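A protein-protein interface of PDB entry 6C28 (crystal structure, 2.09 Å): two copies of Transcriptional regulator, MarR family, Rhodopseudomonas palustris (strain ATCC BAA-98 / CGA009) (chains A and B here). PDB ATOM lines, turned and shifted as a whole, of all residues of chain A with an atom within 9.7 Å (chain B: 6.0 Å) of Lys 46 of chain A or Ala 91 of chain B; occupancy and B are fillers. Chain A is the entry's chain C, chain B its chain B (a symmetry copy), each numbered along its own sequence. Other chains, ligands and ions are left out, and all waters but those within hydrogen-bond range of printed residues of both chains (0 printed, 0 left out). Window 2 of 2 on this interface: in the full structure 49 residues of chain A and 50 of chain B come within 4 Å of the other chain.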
ATOM      1  N   GLU A  44      23.932 -33.394  -6.493  1.00  0.00           N
ATOM      2  CA  GLU A  44      23.196 -32.149  -6.184  1.00  0.00           C
ATOM      3  C   GLU A  44      24.179 -31.025  -6.039  1.00  0.00           C
ATOM      4  O   GLU A  44      25.215 -31.190  -5.401  1.00  0.00           O
ATOM      5  CB  GLU A  44      22.424 -32.307  -4.872  1.00  0.00           C
ATOM      6  N   LEU A  45      23.762 -29.852  -6.492  1.00  0.00           N
ATOM      7  CA  LEU A  45      24.518 -28.627  -6.429  1.00  0.00           C
ATOM      8  C   LEU A  45      23.548 -27.457  -6.419  1.00  0.00           C
ATOM      9  O   LEU A  45      23.750 -26.518  -5.716  1.00  0.00           O
ATOM     10  CB  LEU A  45      25.369 -28.481  -7.640  1.00  0.00           C
ATOM     11  CG  LEU A  45      26.807 -28.805  -7.787  1.00  0.00           C
ATOM     12  CD1 LEU A  45      26.895 -28.166  -9.133  1.00  0.00           C
ATOM     13  CD2 LEU A  45      27.792 -28.169  -6.832  1.00  0.00           C
ATOM     14  N   LYS A  46      22.553 -27.465  -7.284  1.00  0.00           N
ATOM     15  CA  LYS A  46      21.532 -26.410  -7.222  1.00  0.00           C
ATOM     16  C   LYS A  46      20.763 -26.595  -5.921  1.00  0.00           C
ATOM     17  O   LYS A  46      20.306 -27.691  -5.652  1.00  0.00           O
ATOM     18  CB  LYS A  46      20.579 -26.450  -8.418  1.00  0.00           C
ATOM     19  CG  LYS A  46      21.174 -25.901  -9.702  1.00  0.00           C
ATOM     20  CD  LYS A  46      20.155 -26.085 -10.831  1.00  0.00           C
ATOM     21  CE  LYS A  46      20.371 -25.096 -11.954  1.00  0.00           C
ATOM     22  NZ  LYS A  46      19.546 -25.429 -13.151  1.00  0.00           N
ATOM     23  N   MET A  47      20.639 -25.521  -5.134  1.00  0.00           N
ATOM     24  CA  MET A  47      20.108 -25.607  -3.786  1.00  0.00           C
ATOM     25  C   MET A  47      18.675 -25.141  -3.745  1.00  0.00           C
ATOM     26  O   MET A  47      18.008 -25.352  -2.743  1.00  0.00           O
ATOM     27  CB  MET A  47      20.945 -24.807  -2.795  1.00  0.00           C
ATOM     28  CG  MET A  47      22.354 -25.303  -2.581  1.00  0.00           C
ATOM     29  SD  MET A  47      22.457 -27.029  -2.104  1.00  0.00           S
ATOM     30  CE  MET A  47      21.781 -26.969  -0.450  1.00  0.00           C
ATOM     31  N   GLY A  48      18.208 -24.549  -4.849  1.00  0.00           N
ATOM     32  CA  GLY A  48      16.912 -23.938  -4.938  1.00  0.00           C
ATOM     33  C   GLY A  48      16.597 -23.102  -3.709  1.00  0.00           C
ATOM     34  O   GLY A  48      17.457 -22.351  -3.220  1.00  0.00           O
ATOM     35  N   GLU A  49      15.383 -23.312  -3.186  1.00  0.00           N
ATOM     36  CA  GLU A  49      14.881 -22.562  -2.063  1.00  0.00           C
ATOM     37  C   GLU A  49      15.663 -22.831  -0.771  1.00  0.00           C
ATOM     38  O   GLU A  49      15.585 -22.015   0.112  1.00  0.00           O
ATOM     39  CB  GLU A  49      13.393 -22.894  -1.796  1.00  0.00           C
ATOM     40  CG  GLU A  49      12.385 -22.366  -2.816  1.00  0.00           C
ATOM     41  CD  GLU A  49      12.175 -23.293  -4.001  1.00  0.00           C
ATOM     42  OE1 GLU A  49      12.999 -24.209  -4.232  1.00  0.00           O
ATOM     43  OE2 GLU A  49      11.182 -23.101  -4.709  1.00  0.00           O
ATOM     44  N   LEU A  50      16.371 -23.969  -0.649  1.00  0.00           N
ATOM     45  CA  LEU A  50      17.130 -24.307   0.579  1.00  0.00           C
ATOM     46  C   LEU A  50      18.037 -23.207   1.027  1.00  0.00           C
ATOM     47  O   LEU A  50      18.173 -22.949   2.232  1.00  0.00           O
ATOM     48  CB  LEU A  50      18.011 -25.570   0.436  1.00  0.00           C
ATOM     49  CG  LEU A  50      17.468 -26.955   0.833  1.00  0.00           C
ATOM     50  CD1 LEU A  50      16.154 -26.943   1.598  1.00  0.00           C
ATOM     51  CD2 LEU A  50      17.377 -27.891  -0.336  1.00  0.00           C
ATOM     52  N   SER A  51      18.679 -22.561   0.056  1.00  0.00           N
ATOM     53  CA  SER A  51      19.688 -21.569   0.370  1.00  0.00           C
ATOM     54  C   SER A  51      19.077 -20.251   0.846  1.00  0.00           C
ATOM     55  O   SER A  51      19.802 -19.385   1.284  1.00  0.00           O
ATOM     56  CB  SER A  51      20.693 -21.386  -0.798  1.00  0.00           C
ATOM     57  OG  SER A  51      20.080 -20.986  -1.996  1.00  0.00           O
ATOM     58  N   TYR A  56      16.958 -24.434   7.310  1.00  0.00           N
ATOM     59  CA  TYR A  56      18.045 -25.133   6.671  1.00  0.00           C
ATOM     60  C   TYR A  56      19.398 -24.573   7.143  1.00  0.00           C
ATOM     61  O   TYR A  56      20.267 -25.337   7.529  1.00  0.00           O
ATOM     62  CB  TYR A  56      17.983 -24.999   5.168  1.00  0.00           C
ATOM     63  CG  TYR A  56      19.119 -25.730   4.520  1.00  0.00           C
ATOM     64  CD1 TYR A  56      19.193 -27.130   4.593  1.00  0.00           C
ATOM     65  CD2 TYR A  56      20.192 -25.017   3.896  1.00  0.00           C
ATOM     66  CE1 TYR A  56      20.265 -27.805   4.020  1.00  0.00           C
ATOM     67  CE2 TYR A  56      21.265 -25.685   3.297  1.00  0.00           C
ATOM     68  CZ  TYR A  56      21.278 -27.072   3.352  1.00  0.00           C
ATOM     69  OH  TYR A  56      22.313 -27.738   2.828  1.00  0.00           O
ATOM     70  N   LEU B  86      13.725 -34.271  -1.396  1.00  0.00           N
ATOM     71  CA  LEU B  86      12.839 -34.178  -2.530  1.00  0.00           C
ATOM     72  C   LEU B  86      13.128 -32.923  -3.303  1.00  0.00           C
ATOM     73  O   LEU B  86      13.166 -32.935  -4.525  1.00  0.00           O
ATOM     74  CB  LEU B  86      11.355 -34.177  -2.132  1.00  0.00           C
ATOM     75  CG  LEU B  86      10.720 -35.361  -1.409  1.00  0.00           C
ATOM     76  CD1 LEU B  86       9.277 -34.981  -1.120  1.00  0.00           C
ATOM     77  CD2 LEU B  86      10.796 -36.663  -2.182  1.00  0.00           C
ATOM     78  N   LEU B  87      13.345 -31.838  -2.586  1.00  0.00           N
ATOM     79  CA  LEU B  87      13.639 -30.581  -3.206  1.00  0.00           C
ATOM     80  C   LEU B  87      14.976 -30.640  -3.978  1.00  0.00           C
ATOM     81  O   LEU B  87      15.055 -30.097  -5.073  1.00  0.00           O
ATOM     82  CB  LEU B  87      13.559 -29.439  -2.184  1.00  0.00           C
ATOM     83  CG  LEU B  87      13.681 -28.022  -2.750  1.00  0.00           C
ATOM     84  CD1 LEU B  87      13.391 -27.094  -1.610  1.00  0.00           C
ATOM     85  CD2 LEU B  87      15.033 -27.650  -3.370  1.00  0.00           C
ATOM     86  N   LEU B  88      16.006 -31.288  -3.431  1.00  0.00           N
ATOM     87  CA  LEU B  88      17.248 -31.453  -4.164  1.00  0.00           C
ATOM     88  C   LEU B  88      17.089 -32.346  -5.359  1.00  0.00           C
ATOM     89  O   LEU B  88      17.677 -32.055  -6.400  1.00  0.00           O
ATOM     90  CB  LEU B  88      18.346 -32.012  -3.324  1.00  0.00           C
ATOM     91  CG  LEU B  88      18.969 -31.034  -2.384  1.00  0.00           C
ATOM     92  CD1 LEU B  88      20.109 -31.796  -1.745  1.00  0.00           C
ATOM     93  CD2 LEU B  88      19.490 -29.802  -3.089  1.00  0.00           C
ATOM     94  N   LEU B  89      16.277 -33.398  -5.241  1.00  0.00           N
ATOM     95  CA  LEU B  89      16.059 -34.293  -6.358  1.00  0.00           C
ATOM     96  C   LEU B  89      15.388 -33.611  -7.551  1.00  0.00           C
ATOM     97  O   LEU B  89      15.787 -33.806  -8.701  1.00  0.00           O
ATOM     98  CB  LEU B  89      15.236 -35.480  -5.953  1.00  0.00           C
ATOM     99  CG  LEU B  89      15.940 -36.791  -5.621  1.00  0.00           C
ATOM    100  CD1 LEU B  89      17.273 -36.651  -4.971  1.00  0.00           C
ATOM    101  CD2 LEU B  89      15.018 -37.620  -4.727  1.00  0.00           C
ATOM    102  N   ASP B  90      14.366 -32.825  -7.284  1.00  0.00           N
ATOM    103  CA  ASP B  90      13.634 -32.156  -8.340  1.00  0.00           C
ATOM    104  C   ASP B  90      14.541 -31.099  -9.021  1.00  0.00           C
ATOM    105  O   ASP B  90      14.480 -30.915 -10.220  1.00  0.00           O
ATOM    106  CB  ASP B  90      12.402 -31.500  -7.763  1.00  0.00           C
ATOM    107  CG  ASP B  90      11.654 -30.675  -8.775  1.00  0.00           C
ATOM    108  OD1 ASP B  90      10.947 -31.214  -9.647  1.00  0.00           O
ATOM    109  OD2 ASP B  90      11.769 -29.460  -8.685  1.00  0.00           O
ATOM    110  N   ALA B  91      15.379 -30.407  -8.251  1.00  0.00           N
ATOM    111  CA  ALA B  91      16.265 -29.390  -8.821  1.00  0.00           C
ATOM    112  C   ALA B  91      17.545 -29.956  -9.500  1.00  0.00           C
ATOM    113  O   ALA B  91      18.174 -29.267 -10.277  1.00  0.00           O
ATOM    114  CB  ALA B  91      16.621 -28.375  -7.778  1.00  0.00           C
ATOM    115  N   ASN B  92      17.922 -31.188  -9.188  1.00  0.00           N
ATOM    116  CA  ASN B  92      19.155 -31.792  -9.686  1.00  0.00           C
ATOM    117  C   ASN B  92      18.856 -33.230 -10.112  1.00  0.00           C
ATOM    118  O   ASN B  92      19.189 -34.156  -9.403  1.00  0.00           O
ATOM    119  CB  ASN B  92      20.229 -31.827  -8.576  1.00  0.00           C
ATOM    120  CG  ASN B  92      20.639 -30.448  -8.092  1.00  0.00           C
ATOM    121  OD1 ASN B  92      21.524 -29.765  -8.692  1.00  0.00           O
ATOM    122  ND2 ASN B  92      20.083 -30.063  -6.935  1.00  0.00           N
ATOM    123  N   PRO B  93      18.190 -33.421 -11.243  1.00  0.00           N
ATOM    124  CA  PRO B  93      17.855 -34.799 -11.694  1.00  0.00           C
ATOM    125  C   PRO B  93      19.062 -35.626 -12.115  1.00  0.00           C
ATOM    126  O   PRO B  93      20.059 -35.059 -12.550  1.00  0.00           O
ATOM    127  CB  PRO B  93      16.949 -34.559 -12.921  1.00  0.00           C
ATOM    128  CG  PRO B  93      17.361 -33.202 -13.409  1.00  0.00           C
ATOM    129  CD  PRO B  93      17.671 -32.397 -12.172  1.00  0.00           C
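The backbone NH (N) of Leu 45 of chain A sits at hydrogen-bond distance from the side-chain amide oxygen (OD1) of Asn 92 of chain B (3.1 Å).
The backbone carbonyl oxygen (O) of Lys 46 of chain A is in hydrogen-bond range of the side-chain amide nitrogen (ND2) of Asn 92 of chain B, at 2.7 Å.
O of Leu 88 of chain B sits at hydrogen-bond distance from ND2 of Asn 92 of chain B, 3.2 Å away.
Among the printed residues, pairs that only touch across the chains: Lys 46 of chain A with Leu 88 of chain B, Glu 44 of chain A with Asn 92 of chain B, Lys 46 of chain A with Ala 91 of chain B, Met 47 of chain A with Leu 87 of chain B, Leu 50 of chain A with Leu 87 of chain B, Glu 49 of chain A with Leu 87 of chain B, Glu 44 of chain A with Leu 88 of chain B and Leu 50 of chain A with Leu 88 of chain B.
Of the printed residues of chain B, Glu 44 of chain A touches Leu 88 and Asn 92.
Printed residues of chain B within 4 Å of Leu 45 of chain A: Asn 92.
Of the printed residues of chain B, Met 47 of chain A touches Leu 87.
Asp 90 of chain B touches none of the printed residues of chain A.
Of chain A, only Lys 46 (3.8 Å) comes within 4 Å of Ala 91 of chain B.
Of chain A, only Glu 44 (3.6 Å), Leu 45 (3.1 Å) and Lys 46 (2.7 Å) come within 4 Å of Asn 92 of chain B.
The nearest printed residue of chain B that does not touch Met 47 of chain A is Leu 88 of chain B (4.2 Å).
Printed residues of chain A that touch a printed residue of chain B: Glu 44, Leu 45, Lys 46, Met 47, Glu 49 and Leu 50.
Along chain A the printed residues that touch a printed residue of chain B span positions 44 to 50.
Among the printed residues, 10 pairs touch across the chains.
No position is printed for both chains.
Of the 10 pairs that touch across the chains among the printed residues, none has its exchanged pair printed and touching as well.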
